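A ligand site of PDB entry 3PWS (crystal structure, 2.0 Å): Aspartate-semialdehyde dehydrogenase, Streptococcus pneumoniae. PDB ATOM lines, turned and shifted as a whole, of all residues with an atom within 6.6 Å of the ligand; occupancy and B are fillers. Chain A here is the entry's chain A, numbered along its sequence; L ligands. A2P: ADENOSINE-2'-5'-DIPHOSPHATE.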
ATOM      1  N   VAL A   8      14.784  26.457  -3.283  1.00  0.00           N
ATOM      2  CA  VAL A   8      13.569  26.149  -2.533  1.00  0.00           C
ATOM      3  C   VAL A   8      12.590  25.387  -3.420  1.00  0.00           C
ATOM      4  O   VAL A   8      12.111  25.923  -4.425  1.00  0.00           O
ATOM      5  CB  VAL A   8      12.911  27.424  -1.949  1.00  0.00           C
ATOM      6  CG1 VAL A   8      11.690  27.066  -1.099  1.00  0.00           C
ATOM      7  CG2 VAL A   8      13.916  28.210  -1.118  1.00  0.00           C
ATOM      8  N   GLY A   9      12.305  24.144  -3.045  1.00  0.00           N
ATOM      9  CA  GLY A   9      11.517  23.236  -3.863  1.00  0.00           C
ATOM     10  C   GLY A   9      12.429  22.391  -4.746  1.00  0.00           C
ATOM     11  O   GLY A   9      12.109  22.130  -5.909  1.00  0.00           O
ATOM     12  N   ALA A  10      13.545  21.950  -4.171  1.00  0.00           N
ATOM     13  CA  ALA A  10      14.585  21.230  -4.908  1.00  0.00           C
ATOM     14  C   ALA A  10      14.116  19.864  -5.428  1.00  0.00           C
ATOM     15  O   ALA A  10      14.660  19.355  -6.414  1.00  0.00           O
ATOM     16  CB  ALA A  10      15.829  21.060  -4.041  1.00  0.00           C
ATOM     17  N   THR A  11      13.120  19.289  -4.762  1.00  0.00           N
ATOM     18  CA  THR A  11      12.628  17.942  -5.093  1.00  0.00           C
ATOM     19  C   THR A  11      11.606  17.932  -6.230  1.00  0.00           C
ATOM     20  O   THR A  11      11.324  16.872  -6.805  1.00  0.00           O
ATOM     21  CB  THR A  11      12.038  17.244  -3.851  1.00  0.00           C
ATOM     22  OG1 THR A  11      11.039  18.080  -3.252  1.00  0.00           O
ATOM     23  CG2 THR A  11      13.124  16.957  -2.823  1.00  0.00           C
ATOM     24  N   GLY A  12      11.053  19.094  -6.554  1.00  0.00           N
ATOM     25  CA  GLY A  12       9.999  19.206  -7.575  1.00  0.00           C
ATOM     26  C   GLY A  12      10.485  19.102  -9.008  1.00  0.00           C
ATOM     27  O   GLY A  12      11.675  18.918  -9.265  1.00  0.00           O
ATOM     28  N   ALA A  13       9.552  19.217  -9.949  1.00  0.00           N
ATOM     29  CA  ALA A  13       9.837  19.138 -11.379  1.00  0.00           C
ATOM     30  C   ALA A  13      10.734  20.286 -11.854  1.00  0.00           C
ATOM     31  O   ALA A  13      11.724  20.063 -12.556  1.00  0.00           O
ATOM     32  CB  ALA A  13       8.545  19.083 -12.191  1.00  0.00           C
ATOM     33  N   VAL A  14      10.376  21.513 -11.477  1.00  0.00           N
ATOM     34  CA  VAL A  14      11.196  22.697 -11.775  1.00  0.00           C
ATOM     35  C   VAL A  14      12.495  22.666 -10.966  1.00  0.00           C
ATOM     36  O   VAL A  14      13.581  22.922 -11.494  1.00  0.00           O
ATOM     37  CB  VAL A  14      10.427  24.018 -11.522  1.00  0.00           C
ATOM     38  CG1 VAL A  14      11.344  25.224 -11.740  1.00  0.00           C
ATOM     39  CG2 VAL A  14       9.202  24.107 -12.412  1.00  0.00           C
ATOM     40  N   GLY A  15      12.383  22.337  -9.676  1.00  0.00           N
ATOM     41  CA  GLY A  15      13.535  22.245  -8.777  1.00  0.00           C
ATOM     42  C   GLY A  15      14.636  21.344  -9.299  1.00  0.00           C
ATOM     43  O   GLY A  15      15.821  21.670  -9.172  1.00  0.00           O
ATOM     44  N   LEU A  35      16.352  23.172  -0.309  1.00  0.00           N
ATOM     45  CA  LEU A  35      15.258  23.364   0.631  1.00  0.00           C
ATOM     46  C   LEU A  35      13.935  22.824   0.079  1.00  0.00           C
ATOM     47  O   LEU A  35      13.644  22.969  -1.117  1.00  0.00           O
ATOM     48  CB  LEU A  35      15.101  24.847   0.991  1.00  0.00           C
ATOM     49  CG  LEU A  35      15.990  25.493   2.065  1.00  0.00           C
ATOM     50  CD1 LEU A  35      17.467  25.539   1.672  1.00  0.00           C
ATOM     51  CD2 LEU A  35      15.489  26.893   2.357  1.00  0.00           C
ATOM     52  N   ALA A  36      13.152  22.201   0.950  1.00  0.00           N
ATOM     53  CA  ALA A  36      11.832  21.675   0.622  1.00  0.00           C
ATOM     54  C   ALA A  36      10.961  21.627   1.873  1.00  0.00           C
ATOM     55  O   ALA A  36      11.245  22.338   2.849  1.00  0.00           O
ATOM     56  CB  ALA A  36      11.944  20.297  -0.036  1.00  0.00           C
ATOM     57  N   SER A  37       9.902  20.818   1.861  1.00  0.00           N
ATOM     58  CA  SER A  37       9.043  20.666   3.034  1.00  0.00           C
ATOM     59  C   SER A  37       9.665  19.691   4.050  1.00  0.00           C
ATOM     60  O   SER A  37      10.658  19.023   3.739  1.00  0.00           O
ATOM     61  CB  SER A  37       7.634  20.223   2.642  1.00  0.00           C
ATOM     62  OG  SER A  37       7.601  18.867   2.224  1.00  0.00           O
ATOM     63  N   ALA A  38       9.059  19.611   5.231  1.00  0.00           N
ATOM     64  CA  ALA A  38       9.548  18.773   6.335  1.00  0.00           C
ATOM     65  C   ALA A  38       9.739  17.298   5.945  1.00  0.00           C
ATOM     66  O   ALA A  38      10.651  16.638   6.451  1.00  0.00           O
ATOM     67  CB  ALA A  38       8.623  18.884   7.542  1.00  0.00           C
ATOM     68  N   ARG A  39       8.886  16.796   5.054  1.00  0.00           N
ATOM     69  CA  ARG A  39       8.932  15.384   4.657  1.00  0.00           C
ATOM     70  C   ARG A  39      10.122  15.033   3.763  1.00  0.00           C
ATOM     71  O   ARG A  39      10.490  13.863   3.640  1.00  0.00           O
ATOM     72  CB  ARG A  39       7.603  14.956   4.003  1.00  0.00           C
ATOM     73  CG  ARG A  39       7.319  15.585   2.645  1.00  0.00           C
ATOM     74  CD  ARG A  39       6.105  14.943   1.982  1.00  0.00           C
ATOM     75  NE  ARG A  39       5.785  15.578   0.703  1.00  0.00           N
ATOM     76  CZ  ARG A  39       4.728  15.274  -0.055  1.00  0.00           C
ATOM     77  NH1 ARG A  39       3.865  14.337   0.341  1.00  0.00           N
ATOM     78  NH2 ARG A  39       4.533  15.901  -1.201  1.00  0.00           N
ATOM     79  N   SER A  40      10.725  16.051   3.149  1.00  0.00           N
ATOM     80  CA  SER A  40      11.915  15.857   2.321  1.00  0.00           C
ATOM     81  C   SER A  40      13.212  16.080   3.097  1.00  0.00           C
ATOM     82  O   SER A  40      14.275  15.629   2.663  1.00  0.00           O
ATOM     83  CB  SER A  40      11.874  16.771   1.094  1.00  0.00           C
ATOM     84  OG  SER A  40      10.842  16.392   0.205  1.00  0.00           O
ATOM     85  N   ALA A  41      13.124  16.782   4.222  1.00  0.00           N
ATOM     86  CA  ALA A  41      14.280  17.100   5.054  1.00  0.00           C
ATOM     87  C   ALA A  41      14.993  15.836   5.530  1.00  0.00           C
ATOM     88  O   ALA A  41      14.360  14.904   6.033  1.00  0.00           O
ATOM     89  CB  ALA A  41      13.875  17.955   6.239  1.00  0.00           C
ATOM     90  N   ILE A  54      18.899  17.685   2.027  1.00  0.00           N
ATOM     91  CA  ILE A  54      17.723  18.549   1.894  1.00  0.00           C
ATOM     92  C   ILE A  54      17.316  19.098   3.263  1.00  0.00           C
ATOM     93  O   ILE A  54      17.269  18.362   4.248  1.00  0.00           O
ATOM     94  CB  ILE A  54      16.538  17.805   1.242  1.00  0.00           C
ATOM     95  CG1 ILE A  54      16.938  17.320  -0.165  1.00  0.00           C
ATOM     96  CG2 ILE A  54      15.296  18.696   1.166  1.00  0.00           C
ATOM     97  CD1 ILE A  54      16.100  16.161  -0.686  1.00  0.00           C
ATOM     98  N   GLU A  56      14.555  21.634   5.623  1.00  0.00           N
ATOM     99  CA  GLU A  56      13.180  22.134   5.689  1.00  0.00           C
ATOM    100  C   GLU A  56      13.171  23.656   5.593  1.00  0.00           C
ATOM    101  O   GLU A  56      13.941  24.330   6.286  1.00  0.00           O
ATOM    102  CB  GLU A  56      12.495  21.675   6.984  1.00  0.00           C
ATOM    103  CG  GLU A  56      11.056  22.170   7.133  1.00  0.00           C
ATOM    104  CD  GLU A  56      10.444  21.864   8.495  1.00  0.00           C
ATOM    105  OE1 GLU A  56      11.171  21.404   9.399  1.00  0.00           O
ATOM    106  OE2 GLU A  56       9.231  22.087   8.655  1.00  0.00           O
ATOM    107  N   THR A  57      12.308  24.189   4.742  1.00  0.00           N
ATOM    108  CA  THR A  57      12.173  25.626   4.568  1.00  0.00           C
ATOM    109  C   THR A  57      11.480  26.241   5.782  1.00  0.00           C
ATOM    110  O   THR A  57      10.327  25.924   6.088  1.00  0.00           O
ATOM    111  CB  THR A  57      11.386  25.971   3.277  1.00  0.00           C
ATOM    112  OG1 THR A  57      11.885  25.191   2.186  1.00  0.00           O
ATOM    113  CG2 THR A  57      11.517  27.448   2.937  1.00  0.00           C
ATOM    114  N   SER A  71      10.775  27.689  -6.247  1.00  0.00           N
ATOM    115  CA  SER A  71       9.764  27.040  -7.075  1.00  0.00           C
ATOM    116  C   SER A  71       9.040  25.965  -6.281  1.00  0.00           C
ATOM    117  O   SER A  71       9.152  24.768  -6.577  1.00  0.00           O
ATOM    118  CB  SER A  71      10.357  26.476  -8.365  1.00  0.00           C
ATOM    119  OG  SER A  71       9.344  26.333  -9.338  1.00  0.00           O
ATOM    120  N   ALA A  72       8.298  26.408  -5.272  1.00  0.00           N
ATOM    121  CA  ALA A  72       7.635  25.501  -4.350  1.00  0.00           C
ATOM    122  C   ALA A  72       6.158  25.876  -4.141  1.00  0.00           C
ATOM    123  O   ALA A  72       5.586  25.616  -3.083  1.00  0.00           O
ATOM    124  CB  ALA A  72       8.373  25.482  -3.015  1.00  0.00           C
ATOM    125  N   GLY A  73       5.557  26.477  -5.163  1.00  0.00           N
ATOM    126  CA  GLY A  73       4.170  26.926  -5.086  1.00  0.00           C
ATOM    127  C   GLY A  73       4.072  28.296  -4.447  1.00  0.00           C
ATOM    128  O   GLY A  73       4.886  28.649  -3.581  1.00  0.00           O
ATOM    129  N   SER A  75       2.285  29.597  -2.248  1.00  0.00           N
ATOM    130  CA  SER A  75       2.099  29.630  -0.801  1.00  0.00           C
ATOM    131  C   SER A  75       3.428  29.646  -0.043  1.00  0.00           C
ATOM    132  O   SER A  75       3.540  30.294   0.996  1.00  0.00           O
ATOM    133  CB  SER A  75       1.244  28.443  -0.342  1.00  0.00           C
ATOM    134  OG  SER A  75       0.812  28.607   1.000  1.00  0.00           O
ATOM    135  N   THR A  76       4.422  28.936  -0.572  1.00  0.00           N
ATOM    136  CA  THR A  76       5.750  28.875   0.029  1.00  0.00           C
ATOM    137  C   THR A  76       6.492  30.204  -0.150  1.00  0.00           C
ATOM    138  O   THR A  76       7.186  30.668   0.759  1.00  0.00           O
ATOM    139  CB  THR A  76       6.574  27.713  -0.568  1.00  0.00           C
ATOM    140  OG1 THR A  76       5.824  26.499  -0.478  1.00  0.00           O
ATOM    141  CG2 THR A  76       7.889  27.531   0.191  1.00  0.00           C
ATOM    142  N   LYS A  79       5.087  32.957   2.106  1.00  0.00           N
ATOM    143  CA  LYS A  79       5.438  32.753   3.509  1.00  0.00           C
ATOM    144  C   LYS A  79       6.919  32.980   3.840  1.00  0.00           C
ATOM    145  O   LYS A  79       7.237  33.487   4.914  1.00  0.00           O
ATOM    146  CB  LYS A  79       5.027  31.343   3.970  1.00  0.00           C
ATOM    147  CG  LYS A  79       3.529  31.166   4.202  1.00  0.00           C
ATOM    148  CD  LYS A  79       3.207  29.825   4.865  1.00  0.00           C
ATOM    149  CE  LYS A  79       3.290  28.665   3.871  1.00  0.00           C
ATOM    150  NZ  LYS A  79       3.188  27.341   4.551  1.00  0.00           N
ATOM    151  N   TYR A  80       7.808  32.604   2.922  1.00  0.00           N
ATOM    152  CA  TYR A  80       9.238  32.567   3.242  1.00  0.00           C
ATOM    153  C   TYR A  80      10.126  33.560   2.488  1.00  0.00           C
ATOM    154  O   TYR A  80      11.213  33.890   2.965  1.00  0.00           O
ATOM    155  CB  TYR A  80       9.790  31.137   3.115  1.00  0.00           C
ATOM    156  CG  TYR A  80       9.054  30.127   3.971  1.00  0.00           C
ATOM    157  CD1 TYR A  80       9.203  30.127   5.361  1.00  0.00           C
ATOM    158  CD2 TYR A  80       8.215  29.177   3.395  1.00  0.00           C
ATOM    159  CE1 TYR A  80       8.533  29.198   6.154  1.00  0.00           C
ATOM    160  CE2 TYR A  80       7.536  28.253   4.178  1.00  0.00           C
ATOM    161  CZ  TYR A  80       7.694  28.266   5.554  1.00  0.00           C
ATOM    162  OH  TYR A  80       7.027  27.342   6.325  1.00  0.00           O
ATOM    163  N   SER A 158       4.018  18.598 -17.465  1.00  0.00           N
ATOM    164  CA  SER A 158       5.054  18.872 -16.469  1.00  0.00           C
ATOM    165  C   SER A 158       4.912  20.244 -15.816  1.00  0.00           C
ATOM    166  O   SER A 158       5.435  20.483 -14.728  1.00  0.00           O
ATOM    167  CB  SER A 158       6.465  18.711 -17.042  1.00  0.00           C
ATOM    168  OG  SER A 158       6.732  19.667 -18.058  1.00  0.00           O
ATOM    169  N   GLY A 159       4.186  21.148 -16.487  1.00  0.00           N
ATOM    170  CA  GLY A 159       3.878  22.466 -15.952  1.00  0.00           C
ATOM    171  C   GLY A 159       3.098  22.384 -14.651  1.00  0.00           C
ATOM    172  O   GLY A 159       3.268  23.229 -13.764  1.00  0.00           O
ATOM    173  N   ALA A 160       2.255  21.363 -14.530  1.00  0.00           N
ATOM    174  CA  ALA A 160       1.455  21.140 -13.322  1.00  0.00           C
ATOM    175  C   ALA A 160       2.227  20.398 -12.229  1.00  0.00           C
ATOM    176  O   ALA A 160       1.698  20.156 -11.143  1.00  0.00           O
ATOM    177  CB  ALA A 160       0.180  20.399 -13.673  1.00  0.00           C
ATOM    178  N   GLY A 161       3.476  20.037 -12.518  1.00  0.00           N
ATOM    179  CA  GLY A 161       4.330  19.386 -11.530  1.00  0.00           C
ATOM    180  C   GLY A 161       4.583  17.907 -11.785  1.00  0.00           C
ATOM    181  O   GLY A 161       4.061  17.335 -12.736  1.00  0.00           O
ATOM    182  N   MET A 162       5.384  17.302 -10.914  1.00  0.00           N
ATOM    183  CA  MET A 162       5.797  15.912 -11.051  1.00  0.00           C
ATOM    184  C   MET A 162       4.637  14.921 -11.050  1.00  0.00           C
ATOM    185  O   MET A 162       4.647  13.951 -11.815  1.00  0.00           O
ATOM    186  CB  MET A 162       6.804  15.551  -9.956  1.00  0.00           C
ATOM    187  CG  MET A 162       7.667  14.343 -10.286  1.00  0.00           C
ATOM    188  SD  MET A 162       8.936  14.708 -11.505  1.00  0.00           S
ATOM    189  CE  MET A 162      10.192  15.454 -10.463  1.00  0.00           C
ATOM    190  N   GLY A 163       3.650  15.149 -10.182  1.00  0.00           N
ATOM    191  CA  GLY A 163       2.478  14.283 -10.062  1.00  0.00           C
ATOM    192  C   GLY A 163       1.685  14.177 -11.355  1.00  0.00           C
ATOM    193  O   GLY A 163       1.195  13.103 -11.706  1.00  0.00           O
HETATM  194  P1  A2P L   1       8.431  18.266  -1.090  1.00  0.00           P
HETATM  195  O1P A2P L   1       9.026  17.200  -1.981  1.00  0.00           O
HETATM  196  O2P A2P L   1       9.098  18.396   0.256  1.00  0.00           O
HETATM  197  O3P A2P L   1       6.922  18.229  -1.016  1.00  0.00           O
HETATM  198  P2  A2P L   1       6.005  19.531  -7.869  1.00  0.00           P
HETATM  199  O4P A2P L   1       5.780  18.338  -6.967  1.00  0.00           O
HETATM  200  O5P A2P L   1       4.772  20.339  -8.157  1.00  0.00           O
HETATM  201  O6P A2P L   1       6.846  19.223  -9.087  1.00  0.00           O
HETATM  202  O5' A2P L   1       6.943  20.529  -7.005  1.00  0.00           O
HETATM  203  C5' A2P L   1       6.519  21.025  -5.726  1.00  0.00           C
HETATM  204  C4' A2P L   1       7.753  21.358  -4.882  1.00  0.00           C
HETATM  205  O4' A2P L   1       7.420  22.281  -3.844  1.00  0.00           O
HETATM  206  C3' A2P L   1       8.304  20.116  -4.192  1.00  0.00           C
HETATM  207  O3' A2P L   1       9.729  20.140  -4.302  1.00  0.00           O
HETATM  208  C2' A2P L   1       7.898  20.272  -2.744  1.00  0.00           C
HETATM  209  O2' A2P L   1       8.811  19.647  -1.835  1.00  0.00           O
HETATM  210  C1' A2P L   1       7.901  21.786  -2.583  1.00  0.00           C
HETATM  211  N9  A2P L   1       7.047  22.230  -1.450  1.00  0.00           N
HETATM  212  C8  A2P L   1       5.734  22.021  -1.303  1.00  0.00           C
HETATM  213  N7  A2P L   1       5.327  22.581  -0.138  1.00  0.00           N
HETATM  214  C5  A2P L   1       6.402  23.157   0.436  1.00  0.00           C
HETATM  215  C6  A2P L   1       6.593  23.863   1.619  1.00  0.00           C
HETATM  216  N6  A2P L   1       5.551  24.090   2.449  1.00  0.00           N
HETATM  217  N1  A2P L   1       7.838  24.322   1.921  1.00  0.00           N
HETATM  218  C2  A2P L   1       8.880  24.089   1.099  1.00  0.00           C
HETATM  219  N3  A2P L   1       8.721  23.401  -0.045  1.00  0.00           N
HETATM  220  C4  A2P L   1       7.486  22.929  -0.393  1.00  0.00           C
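OG1 of Thr 11 is in hydrogen-bond range of O1P of the ligand.
NH2 of Arg 39 lies within salt-bridge range of O3P of the ligand (3.3 Å).
The backbone NH (N) of Ala 13 is in hydrogen-bond range of an oxygen (O6P) of the ligand, 2.8 Å away.
O of Gly 9 lies within hydrogen-bond range of O3' of the ligand (3.5 Å).
O2P of the ligand lies within hydrogen-bond range of OG of Ser 37, 2.5 Å away.
The backbone NH (N) of Ser 37 sits at hydrogen-bond distance from an oxygen (O2P) of the ligand (3.0 Å).
O2P of the ligand sits at hydrogen-bond distance from OG of Ser 40, 2.7 Å away.
N of Gly 12 is in hydrogen-bond range of O3' of the ligand (2.8 Å).
The backbone NH of Met 162 sits at hydrogen-bond distance from an oxygen (O6P) of the ligand (3.0 Å).
O of Ala 36 lies within hydrogen-bond range of N of Thr 57 (2.9 Å).
The backbone NH of Gly 9 is in hydrogen-bond range of the backbone carbonyl oxygen of Leu 35, 2.6 Å away.
O of Ala 72 sits at hydrogen-bond distance from OG1 of Thr 76 (2.8 Å).
Merely in contact with the ligand: Ala 72, Ala 36, Thr 57, Thr 76 and Gly 161.
Hydrophobic or aromatic side chains within 4 Å of the ligand: Ala 13, Ala 36, Ala 72 and Met 162.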
